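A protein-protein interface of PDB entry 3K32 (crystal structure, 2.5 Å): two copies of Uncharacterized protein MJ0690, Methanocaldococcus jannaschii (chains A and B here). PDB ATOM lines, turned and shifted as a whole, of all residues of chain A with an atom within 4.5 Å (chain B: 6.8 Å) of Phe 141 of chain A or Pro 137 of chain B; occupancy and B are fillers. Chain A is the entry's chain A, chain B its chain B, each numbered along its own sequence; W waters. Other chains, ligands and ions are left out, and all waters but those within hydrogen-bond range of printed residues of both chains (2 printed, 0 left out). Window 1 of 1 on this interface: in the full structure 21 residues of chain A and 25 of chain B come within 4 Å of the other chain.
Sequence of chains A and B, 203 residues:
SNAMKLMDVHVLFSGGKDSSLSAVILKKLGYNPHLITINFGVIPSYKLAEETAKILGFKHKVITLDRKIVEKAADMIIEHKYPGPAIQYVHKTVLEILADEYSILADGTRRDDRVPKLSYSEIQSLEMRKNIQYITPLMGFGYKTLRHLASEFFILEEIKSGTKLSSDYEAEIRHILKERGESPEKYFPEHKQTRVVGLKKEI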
ATOM      1  N   ARG A 111      21.362  36.584 -30.085  1.00  0.00           N
ATOM      2  CA  ARG A 111      21.631  36.331 -31.494  1.00  0.00           C
ATOM      3  C   ARG A 111      20.771  37.209 -32.401  1.00  0.00           C
ATOM      4  O   ARG A 111      21.283  37.880 -33.295  1.00  0.00           O
ATOM      5  CB  ARG A 111      21.371  34.864 -31.839  1.00  0.00           C
ATOM      6  CG  ARG A 111      21.825  34.495 -33.251  1.00  0.00           C
ATOM      7  CD  ARG A 111      21.417  33.077 -33.632  1.00  0.00           C
ATOM      8  NE  ARG A 111      20.054  33.029 -34.149  1.00  0.00           N
ATOM      9  CZ  ARG A 111      19.334  31.916 -34.260  1.00  0.00           C
ATOM     10  NH1 ARG A 111      19.850  30.751 -33.870  1.00  0.00           N
ATOM     11  NH2 ARG A 111      18.093  31.979 -34.746  1.00  0.00           N
ATOM     12  N   PRO A 137      26.198  35.588 -23.228  1.00  0.00           N
ATOM     13  CA  PRO A 137      25.841  34.163 -23.202  1.00  0.00           C
ATOM     14  C   PRO A 137      24.740  33.822 -24.191  1.00  0.00           C
ATOM     15  O   PRO A 137      24.691  32.680 -24.658  1.00  0.00           O
ATOM     16  CB  PRO A 137      25.349  33.940 -21.767  1.00  0.00           C
ATOM     17  CG  PRO A 137      25.886  35.114 -20.968  1.00  0.00           C
ATOM     18  CD  PRO A 137      25.929  36.262 -21.948  1.00  0.00           C
ATOM     19  N   LEU A 138      23.882  34.794 -24.503  1.00  0.00           N
ATOM     20  CA  LEU A 138      22.729  34.538 -25.361  1.00  0.00           C
ATOM     21  C   LEU A 138      23.078  34.657 -26.846  1.00  0.00           C
ATOM     22  O   LEU A 138      22.247  34.415 -27.712  1.00  0.00           O
ATOM     23  CB  LEU A 138      21.560  35.465 -25.003  1.00  0.00           C
ATOM     24  CG  LEU A 138      21.132  35.481 -23.529  1.00  0.00           C
ATOM     25  CD1 LEU A 138      19.815  36.266 -23.354  1.00  0.00           C
ATOM     26  CD2 LEU A 138      20.975  34.088 -23.011  1.00  0.00           C
ATOM     27  N   MET A 139      24.317  35.026 -27.130  1.00  0.00           N
ATOM     28  CA  MET A 139      24.726  35.278 -28.494  1.00  0.00           C
ATOM     29  C   MET A 139      24.434  34.080 -29.399  1.00  0.00           C
ATOM     30  O   MET A 139      24.011  34.236 -30.543  1.00  0.00           O
ATOM     31  CB  MET A 139      26.201  35.692 -28.556  1.00  0.00           C
ATOM     32  CG  MET A 139      26.588  36.369 -29.866  1.00  0.00           C
ATOM     33  SD  MET A 139      25.501  37.959 -30.347  1.00  0.00           S
ATOM     34  CE  MET A 139      24.828  37.309 -32.046  1.00  0.00           C
ATOM     35  N   GLY A 140      24.634  32.880 -28.878  1.00  0.00           N
ATOM     36  CA  GLY A 140      24.436  31.686 -29.682  1.00  0.00           C
ATOM     37  C   GLY A 140      23.025  31.127 -29.673  1.00  0.00           C
ATOM     38  O   GLY A 140      22.781  30.042 -30.203  1.00  0.00           O
ATOM     39  N   PHE A 141      22.092  31.869 -29.088  1.00  0.00           N
ATOM     40  CA  PHE A 141      20.748  31.340 -28.840  1.00  0.00           C
ATOM     41  C   PHE A 141      19.648  32.093 -29.575  1.00  0.00           C
ATOM     42  O   PHE A 141      19.359  33.251 -29.270  1.00  0.00           O
ATOM     43  CB  PHE A 141      20.464  31.333 -27.345  1.00  0.00           C
ATOM     44  CG  PHE A 141      21.326  30.379 -26.581  1.00  0.00           C
ATOM     45  CD1 PHE A 141      22.611  30.719 -26.229  1.00  0.00           C
ATOM     46  CD2 PHE A 141      20.860  29.119 -26.252  1.00  0.00           C
ATOM     47  CE1 PHE A 141      23.405  29.823 -25.544  1.00  0.00           C
ATOM     48  CE2 PHE A 141      21.651  28.225 -25.562  1.00  0.00           C
ATOM     49  CZ  PHE A 141      22.924  28.577 -25.206  1.00  0.00           C
ATOM     50  N   GLY A 142      19.033  31.426 -30.546  1.00  0.00           N
ATOM     51  CA  GLY A 142      17.934  32.019 -31.277  1.00  0.00           C
ATOM     52  C   GLY A 142      16.655  32.179 -30.470  1.00  0.00           C
ATOM     53  O   GLY A 142      16.516  31.654 -29.357  1.00  0.00           O
ATOM     54  N   TYR A 143      15.722  32.919 -31.060  1.00  0.00           N
ATOM     55  CA  TYR A 143      14.423  33.208 -30.466  1.00  0.00           C
ATOM     56  C   TYR A 143      13.693  31.975 -29.952  1.00  0.00           C
ATOM     57  O   TYR A 143      13.226  31.974 -28.807  1.00  0.00           O
ATOM     58  CB  TYR A 143      13.543  33.935 -31.474  1.00  0.00           C
ATOM     59  CG  TYR A 143      12.130  34.118 -31.002  1.00  0.00           C
ATOM     60  CD1 TYR A 143      11.124  33.248 -31.403  1.00  0.00           C
ATOM     61  CD2 TYR A 143      11.796  35.170 -30.151  1.00  0.00           C
ATOM     62  CE1 TYR A 143       9.826  33.417 -30.965  1.00  0.00           C
ATOM     63  CE2 TYR A 143      10.508  35.351 -29.712  1.00  0.00           C
ATOM     64  CZ  TYR A 143       9.521  34.472 -30.112  1.00  0.00           C
ATOM     65  OH  TYR A 143       8.228  34.648 -29.654  1.00  0.00           O
ATOM     66  N   THR A 145      14.824  29.043 -29.096  1.00  0.00           N
ATOM     67  CA  THR A 145      15.545  28.375 -28.032  1.00  0.00           C
ATOM     68  C   THR A 145      15.390  29.154 -26.740  1.00  0.00           C
ATOM     69  O   THR A 145      15.107  28.586 -25.695  1.00  0.00           O
ATOM     70  CB  THR A 145      17.041  28.266 -28.389  1.00  0.00           C
ATOM     71  OG1 THR A 145      17.168  27.869 -29.755  1.00  0.00           O
ATOM     72  CG2 THR A 145      17.749  27.245 -27.501  1.00  0.00           C
ATOM     73  N   LEU A 146      15.616  30.460 -26.819  1.00  0.00           N
ATOM     74  CA  LEU A 146      15.351  31.353 -25.706  1.00  0.00           C
ATOM     75  C   LEU A 146      13.917  31.132 -25.223  1.00  0.00           C
ATOM     76  O   LEU A 146      13.644  31.066 -24.026  1.00  0.00           O
ATOM     77  CB  LEU A 146      15.511  32.804 -26.145  1.00  0.00           C
ATOM     78  CG  LEU A 146      16.847  33.505 -25.962  1.00  0.00           C
ATOM     79  CD1 LEU A 146      17.882  32.579 -25.367  1.00  0.00           C
ATOM     80  CD2 LEU A 146      17.320  34.100 -27.270  1.00  0.00           C
ATOM     81  N   LEU A 149      13.709  28.016 -23.261  1.00  0.00           N
ATOM     82  CA  LEU A 149      14.498  28.007 -22.036  1.00  0.00           C
ATOM     83  C   LEU A 149      13.892  28.856 -20.916  1.00  0.00           C
ATOM     84  O   LEU A 149      14.015  28.526 -19.739  1.00  0.00           O
ATOM     85  CB  LEU A 149      15.932  28.457 -22.326  1.00  0.00           C
ATOM     86  CG  LEU A 149      16.868  27.467 -23.036  1.00  0.00           C
ATOM     87  CD1 LEU A 149      18.020  28.210 -23.700  1.00  0.00           C
ATOM     88  CD2 LEU A 149      17.387  26.359 -22.099  1.00  0.00           C
ATOM     89  N   VAL B  11      24.663  17.223 -30.879  1.00  0.00           N
ATOM     90  CA  VAL B  11      25.820  18.097 -30.819  1.00  0.00           C
ATOM     91  C   VAL B  11      26.990  17.547 -31.624  1.00  0.00           C
ATOM     92  O   VAL B  11      27.605  16.558 -31.240  1.00  0.00           O
ATOM     93  CB  VAL B  11      26.306  18.237 -29.372  1.00  0.00           C
ATOM     94  CG1 VAL B  11      27.371  19.328 -29.266  1.00  0.00           C
ATOM     95  CG2 VAL B  11      25.153  18.504 -28.431  1.00  0.00           C
ATOM     96  N   LEU B  21      32.937  21.804 -23.650  1.00  0.00           N
ATOM     97  CA  LEU B  21      32.230  22.889 -22.990  1.00  0.00           C
ATOM     98  C   LEU B  21      30.844  23.081 -23.590  1.00  0.00           C
ATOM     99  O   LEU B  21      29.881  23.351 -22.854  1.00  0.00           O
ATOM    100  CB  LEU B  21      33.015  24.205 -23.061  1.00  0.00           C
ATOM    101  CG  LEU B  21      34.232  24.340 -22.147  1.00  0.00           C
ATOM    102  CD1 LEU B  21      34.832  25.737 -22.262  1.00  0.00           C
ATOM    103  CD2 LEU B  21      33.867  24.013 -20.705  1.00  0.00           C
ATOM    104  N   SER B  22      30.719  22.947 -24.913  1.00  0.00           N
ATOM    105  CA  SER B  22      29.390  23.119 -25.499  1.00  0.00           C
ATOM    106  C   SER B  22      28.439  22.048 -24.963  1.00  0.00           C
ATOM    107  O   SER B  22      27.324  22.356 -24.553  1.00  0.00           O
ATOM    108  CB  SER B  22      29.402  23.169 -27.038  1.00  0.00           C
ATOM    109  OG  SER B  22      29.701  21.914 -27.614  1.00  0.00           O
ATOM    110  N   ALA B  23      28.898  20.798 -24.961  1.00  0.00           N
ATOM    111  CA  ALA B  23      28.127  19.688 -24.403  1.00  0.00           C
ATOM    112  C   ALA B  23      27.654  20.057 -23.005  1.00  0.00           C
ATOM    113  O   ALA B  23      26.457  20.117 -22.736  1.00  0.00           O
ATOM    114  CB  ALA B  23      28.978  18.422 -24.341  1.00  0.00           C
ATOM    115  N   ILE B  25      27.540  22.805 -21.350  1.00  0.00           N
ATOM    116  CA  ILE B  25      26.602  23.893 -21.227  1.00  0.00           C
ATOM    117  C   ILE B  25      25.190  23.443 -21.579  1.00  0.00           C
ATOM    118  O   ILE B  25      24.251  23.698 -20.823  1.00  0.00           O
ATOM    119  CB  ILE B  25      27.045  25.085 -22.062  1.00  0.00           C
ATOM    120  CG1 ILE B  25      28.344  25.630 -21.467  1.00  0.00           C
ATOM    121  CG2 ILE B  25      25.949  26.149 -22.109  1.00  0.00           C
ATOM    122  CD1 ILE B  25      29.007  26.690 -22.323  1.00  0.00           C
ATOM    123  N   LEU B  26      25.038  22.760 -22.714  1.00  0.00           N
ATOM    124  CA  LEU B  26      23.720  22.277 -23.113  1.00  0.00           C
ATOM    125  C   LEU B  26      23.109  21.485 -21.954  1.00  0.00           C
ATOM    126  O   LEU B  26      21.932  21.681 -21.599  1.00  0.00           O
ATOM    127  CB  LEU B  26      23.820  21.414 -24.370  1.00  0.00           C
ATOM    128  CG  LEU B  26      23.567  22.049 -25.761  1.00  0.00           C
ATOM    129  CD1 LEU B  26      23.290  23.568 -25.741  1.00  0.00           C
ATOM    130  CD2 LEU B  26      24.681  21.709 -26.750  1.00  0.00           C
ATOM    131  N   LEU B  29      21.766  23.514 -19.196  1.00  0.00           N
ATOM    132  CA  LEU B  29      20.492  24.154 -19.516  1.00  0.00           C
ATOM    133  C   LEU B  29      19.292  23.203 -19.539  1.00  0.00           C
ATOM    134  O   LEU B  29      18.166  23.613 -19.833  1.00  0.00           O
ATOM    135  CB  LEU B  29      20.595  24.910 -20.840  1.00  0.00           C
ATOM    136  CG  LEU B  29      21.698  25.970 -20.847  1.00  0.00           C
ATOM    137  CD1 LEU B  29      21.884  26.551 -22.238  1.00  0.00           C
ATOM    138  CD2 LEU B  29      21.426  27.076 -19.831  1.00  0.00           C
ATOM    139  N   TYR B  31      19.133  20.196 -21.384  1.00  0.00           N
ATOM    140  CA  TYR B  31      19.002  19.377 -22.587  1.00  0.00           C
ATOM    141  C   TYR B  31      19.634  18.019 -22.417  1.00  0.00           C
ATOM    142  O   TYR B  31      20.629  17.873 -21.713  1.00  0.00           O
ATOM    143  CB  TYR B  31      19.694  20.020 -23.771  1.00  0.00           C
ATOM    144  CG  TYR B  31      19.060  21.284 -24.281  1.00  0.00           C
ATOM    145  CD1 TYR B  31      18.005  21.237 -25.154  1.00  0.00           C
ATOM    146  CD2 TYR B  31      19.558  22.527 -23.924  1.00  0.00           C
ATOM    147  CE1 TYR B  31      17.443  22.380 -25.635  1.00  0.00           C
ATOM    148  CE2 TYR B  31      18.994  23.676 -24.400  1.00  0.00           C
ATOM    149  CZ  TYR B  31      17.937  23.601 -25.262  1.00  0.00           C
ATOM    150  OH  TYR B  31      17.356  24.749 -25.758  1.00  0.00           O
ATOM    151  N   ALA B 106      23.311  21.363 -32.486  1.00  0.00           N
ATOM    152  CA  ALA B 106      24.273  22.221 -31.816  1.00  0.00           C
ATOM    153  C   ALA B 106      25.683  21.882 -32.286  1.00  0.00           C
ATOM    154  O   ALA B 106      25.938  20.748 -32.714  1.00  0.00           O
ATOM    155  CB  ALA B 106      24.166  22.063 -30.308  1.00  0.00           C
ATOM    156  N   ASP B 107      26.594  22.857 -32.199  1.00  0.00           N
ATOM    157  CA  ASP B 107      28.003  22.581 -32.448  1.00  0.00           C
ATOM    158  C   ASP B 107      28.883  23.440 -31.553  1.00  0.00           C
ATOM    159  O   ASP B 107      28.386  24.094 -30.645  1.00  0.00           O
ATOM    160  CB  ASP B 107      28.348  22.787 -33.920  1.00  0.00           C
ATOM    161  CG  ASP B 107      28.307  24.253 -34.331  1.00  0.00           C
ATOM    162  OD1 ASP B 107      28.446  25.127 -33.448  1.00  0.00           O
ATOM    163  OD2 ASP B 107      28.135  24.527 -35.541  1.00  0.00           O
ATOM    164  N   GLY B 108      30.188  23.448 -31.830  1.00  0.00           N
ATOM    165  CA  GLY B 108      31.177  24.049 -30.944  1.00  0.00           C
ATOM    166  C   GLY B 108      31.827  25.304 -31.487  1.00  0.00           C
ATOM    167  O   GLY B 108      32.916  25.703 -31.049  1.00  0.00           O
ATOM    168  N   THR B 109      31.153  25.925 -32.448  1.00  0.00           N
ATOM    169  CA  THR B 109      31.560  27.214 -32.995  1.00  0.00           C
ATOM    170  C   THR B 109      31.614  28.311 -31.928  1.00  0.00           C
ATOM    171  O   THR B 109      30.783  28.365 -31.018  1.00  0.00           O
ATOM    172  CB  THR B 109      30.615  27.642 -34.108  1.00  0.00           C
ATOM    173  OG1 THR B 109      30.655  26.652 -35.139  1.00  0.00           O
ATOM    174  CG2 THR B 109      31.089  28.972 -34.689  1.00  0.00           C
ATOM    175  N   ARG B 110      32.594  29.190 -32.038  1.00  0.00           N
ATOM    176  CA  ARG B 110      32.845  30.122 -30.957  1.00  0.00           C
ATOM    177  C   ARG B 110      33.206  31.509 -31.485  1.00  0.00           C
ATOM    178  O   ARG B 110      33.590  31.657 -32.640  1.00  0.00           O
ATOM    179  CB  ARG B 110      33.942  29.562 -30.056  1.00  0.00           C
ATOM    180  CG  ARG B 110      35.245  29.312 -30.794  1.00  0.00           C
ATOM    181  CD  ARG B 110      36.142  28.286 -30.097  1.00  0.00           C
ATOM    182  NE  ARG B 110      35.721  26.938 -30.442  1.00  0.00           N
ATOM    183  CZ  ARG B 110      36.520  25.996 -30.926  1.00  0.00           C
ATOM    184  NH1 ARG B 110      37.804  26.242 -31.101  1.00  0.00           N
ATOM    185  NH2 ARG B 110      36.026  24.799 -31.217  1.00  0.00           N
ATOM    186  N   TYR B 134      19.118  25.753 -34.465  1.00  0.00           N
ATOM    187  CA  TYR B 134      20.576  25.704 -34.461  1.00  0.00           C
ATOM    188  C   TYR B 134      21.114  26.503 -33.251  1.00  0.00           C
ATOM    189  O   TYR B 134      20.804  27.689 -33.088  1.00  0.00           O
ATOM    190  CB  TYR B 134      21.086  26.309 -35.766  1.00  0.00           C
ATOM    191  CG  TYR B 134      22.594  26.308 -35.932  1.00  0.00           C
ATOM    192  CD1 TYR B 134      23.326  25.119 -35.883  1.00  0.00           C
ATOM    193  CD2 TYR B 134      23.282  27.488 -36.186  1.00  0.00           C
ATOM    194  CE1 TYR B 134      24.694  25.122 -36.059  1.00  0.00           C
ATOM    195  CE2 TYR B 134      24.666  27.492 -36.358  1.00  0.00           C
ATOM    196  CZ  TYR B 134      25.355  26.310 -36.298  1.00  0.00           C
ATOM    197  OH  TYR B 134      26.707  26.322 -36.452  1.00  0.00           O
ATOM    198  N   ILE B 135      21.907  25.846 -32.408  1.00  0.00           N
ATOM    199  CA  ILE B 135      22.376  26.432 -31.151  1.00  0.00           C
ATOM    200  C   ILE B 135      23.890  26.442 -31.026  1.00  0.00           C
ATOM    201  O   ILE B 135      24.521  25.408 -31.134  1.00  0.00           O
ATOM    202  CB  ILE B 135      21.838  25.667 -29.940  1.00  0.00           C
ATOM    203  CG1 ILE B 135      20.303  25.674 -29.947  1.00  0.00           C
ATOM    204  CG2 ILE B 135      22.448  26.254 -28.650  1.00  0.00           C
ATOM    205  CD1 ILE B 135      19.675  24.719 -28.963  1.00  0.00           C
ATOM    206  N   THR B 136      24.473  27.611 -30.785  1.00  0.00           N
ATOM    207  CA  THR B 136      25.924  27.712 -30.654  1.00  0.00           C
ATOM    208  C   THR B 136      26.318  28.318 -29.305  1.00  0.00           C
ATOM    209  O   THR B 136      26.568  29.522 -29.161  1.00  0.00           O
ATOM    210  CB  THR B 136      26.540  28.472 -31.832  1.00  0.00           C
ATOM    211  OG1 THR B 136      26.010  29.796 -31.856  1.00  0.00           O
ATOM    212  CG2 THR B 136      26.181  27.751 -33.158  1.00  0.00           C
ATOM    213  N   PRO B 137      26.369  27.458 -28.302  1.00  0.00           N
ATOM    214  CA  PRO B 137      26.581  27.847 -26.916  1.00  0.00           C
ATOM    215  C   PRO B 137      27.812  28.750 -26.762  1.00  0.00           C
ATOM    216  O   PRO B 137      27.785  29.682 -25.969  1.00  0.00           O
ATOM    217  CB  PRO B 137      26.781  26.508 -26.226  1.00  0.00           C
ATOM    218  CG  PRO B 137      26.091  25.541 -27.064  1.00  0.00           C
ATOM    219  CD  PRO B 137      26.274  26.001 -28.461  1.00  0.00           C
ATOM    220  N   LEU B 138      28.861  28.497 -27.536  1.00  0.00           N
ATOM    221  CA  LEU B 138      30.124  29.204 -27.357  1.00  0.00           C
ATOM    222  C   LEU B 138      30.181  30.542 -28.113  1.00  0.00           C
ATOM    223  O   LEU B 138      31.116  31.335 -27.947  1.00  0.00           O
ATOM    224  CB  LEU B 138      31.286  28.297 -27.787  1.00  0.00           C
ATOM    225  CG  LEU B 138      31.271  26.864 -27.225  1.00  0.00           C
ATOM    226  CD1 LEU B 138      32.506  26.092 -27.684  1.00  0.00           C
ATOM    227  CD2 LEU B 138      31.148  26.830 -25.684  1.00  0.00           C
ATOM    228  N   MET B 139      29.189  30.801 -28.952  1.00  0.00           N
ATOM    229  CA  MET B 139      29.266  31.987 -29.810  1.00  0.00           C
ATOM    230  C   MET B 139      29.499  33.263 -29.004  1.00  0.00           C
ATOM    231  O   MET B 139      30.176  34.171 -29.468  1.00  0.00           O
ATOM    232  CB  MET B 139      28.023  32.131 -30.715  1.00  0.00           C
ATOM    233  CG  MET B 139      28.222  33.128 -31.841  1.00  0.00           C
ATOM    234  SD  MET B 139      29.759  32.740 -33.019  1.00  0.00           S
ATOM    235  CE  MET B 139      29.298  30.942 -33.483  1.00  0.00           C
ATOM    236  N   GLY B 140      28.932  33.331 -27.802  1.00  0.00           N
ATOM    237  CA  GLY B 140      29.100  34.516 -26.977  1.00  0.00           C
ATOM    238  C   GLY B 140      30.349  34.569 -26.106  1.00  0.00           C
ATOM    239  O   GLY B 140      30.519  35.512 -25.348  1.00  0.00           O
ATOM    240  N   PHE B 141      31.218  33.566 -26.218  1.00  0.00           N
ATOM    241  CA  PHE B 141      32.395  33.435 -25.350  1.00  0.00           C
ATOM    242  C   PHE B 141      33.700  33.546 -26.115  1.00  0.00           C
ATOM    243  O   PHE B 141      33.902  32.888 -27.122  1.00  0.00           O
ATOM    244  CB  PHE B 141      32.356  32.104 -24.603  1.00  0.00           C
ATOM    245  CG  PHE B 141      31.130  31.930 -23.778  1.00  0.00           C
ATOM    246  CD1 PHE B 141      29.921  31.606 -24.370  1.00  0.00           C
ATOM    247  CD2 PHE B 141      31.169  32.119 -22.411  1.00  0.00           C
ATOM    248  CE1 PHE B 141      28.770  31.460 -23.600  1.00  0.00           C
ATOM    249  CE2 PHE B 141      30.024  31.986 -21.640  1.00  0.00           C
ATOM    250  CZ  PHE B 141      28.826  31.656 -22.234  1.00  0.00           C
ATOM    251  N   LEU B 146      36.870  31.147 -22.576  1.00  0.00           N
ATOM    252  CA  LEU B 146      36.874  29.708 -22.814  1.00  0.00           C
ATOM    253  C   LEU B 146      38.081  29.034 -22.184  1.00  0.00           C
ATOM    254  O   LEU B 146      37.974  27.920 -21.654  1.00  0.00           O
ATOM    255  CB  LEU B 146      36.870  29.405 -24.316  1.00  0.00           C
ATOM    256  CG  LEU B 146      35.574  29.136 -25.095  1.00  0.00           C
ATOM    257  CD1 LEU B 146      34.330  29.687 -24.421  1.00  0.00           C
ATOM    258  CD2 LEU B 146      35.686  29.654 -26.533  1.00  0.00           C
HETATM  259  O   HOH W   1      26.375  32.060 -26.703  1.00  0.00           O
HETATM  260  O   HOH W   2      19.211  28.683 -31.235  1.00  0.00           O
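The backbone carbonyl oxygen (O) of Gly 140 of chain A is in hydrogen-bond range of the backbone NH (N) of Thr 136 of chain B, at 3.0 Å.
NH1 of Arg 111 of chain A lies within hydrogen-bond range of O of Tyr 134 of chain B (3.3 Å).
Of the printed residues of chain B, Phe 141 of chain A touches Leu 29, Ile 135 and Pro 137.
Of the printed residues of chain A, Pro 137 of chain B touches Phe 141 (3.98 Å).
Of chain B, only Ile 135 (3.8 Å), Thr 136 (3.0 Å) and Met 139 (3.8 Å) come within 4 Å of Gly 140 of chain A.
Printed residues of chain A within 4 Å of Thr 136 of chain B: Gly 140 (3.0 Å).
Of the printed residues of chain A, Ile 135 of chain B touches Gly 140 (3.8 Å), Phe 141 (3.7 Å) and Thr 145 (3.5 Å).
Printed residues of chain A within 4 Å of Leu 29 of chain B: Phe 141 and Leu 149.
The nearest printed residue of chain B that does not touch Thr 145 of chain A is Tyr 134 of chain B (4.9 Å).
Gly 140 of chain B touches Met 139 of chain A (CA to CB, 3.5 Å).
Ile 135 of chain B touches Gly 140 of chain A.
Gly 140 of chain A touches Met 139 of chain B.
Phe 141 of chain A touches Leu 29 of chain B (CE2 to CD1, 3.7 Å).
Ile 135 of chain B touches Phe 141 of chain A (CG2 to CE2, 3.7 Å).
CA of Pro 137 of chain B touches CE1 of Phe 141 of chain A (3.98 Å).
OH of Tyr 31 of chain B touches CG2 of Thr 145 of chain A (3.1 Å).
CD1 of Ile 135 of chain B touches CG2 of Thr 145 of chain A, at 3.5 Å.
Leu 29 of chain B touches Leu 149 of chain A.
Leu 149 of chain A touches Tyr 31 of chain B (CG to OH, 3.9 Å).
Of the 11 printed residues of chain A, 6 touch a printed residue of chain B.
Hydrophobic or aromatic side chains of chain B within 4 Å of the printed part of chain A: Leu 29, Tyr 31, Ile 135 and Met 139.
Among the printed residues, no Asp or Glu carboxylate lies within 4 Å of a Lys or Arg side-chain nitrogen of the other chain.
Met 139 of chain A touches Gly 140 of chain B, and with the chains exchanged Gly 140 of chain A touches Met 139 of chain B.
Phe 141 of chain A touches Pro 137 of chain B, but with the chains exchanged Pro 137 of chain A does not touch Phe 141 of chain B (4.01 Å).
Of the 12 pairs that touch across the chains among the printed residues, 2 have their exchanged pair printed and touching as well.
Water W2 lies within hydrogen-bond range of O of Tyr 134 of chain B (2.6 Å), OG1 of Thr 145 of chain A (2.7 Å), N of Gly 142 of chain A (2.8 Å) and NH1 of Arg 111 of chain A (3.4 Å).
Water W1 lies within hydrogen-bond range of O of Pro 137 of chain A (2.7 Å), O of Pro 137 of chain B (2.9 Å), N of Gly 140 of chain A (2.9 Å) and N of Gly 140 of chain B (3.1 Å).
N of Arg 111 of chain A lies within hydrogen-bond range of O of Leu 138 of chain A, 3.3 Å away.
The side-chain carboxylate (OD2) of Asp 107 of chain B lies within hydrogen-bond range of the side-chain hydroxyl (OH) of Tyr 134 of chain B (2.5 Å).
The backbone carbonyl oxygen of Ile 135 of chain B is in hydrogen-bond range of the backbone NH of Asp 107 of chain B, 3.5 Å away.
The backbone carbonyl oxygen (O) of Leu 26 of chain B sits at hydrogen-bond distance from the backbone NH (N) of Tyr 31 of chain B.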
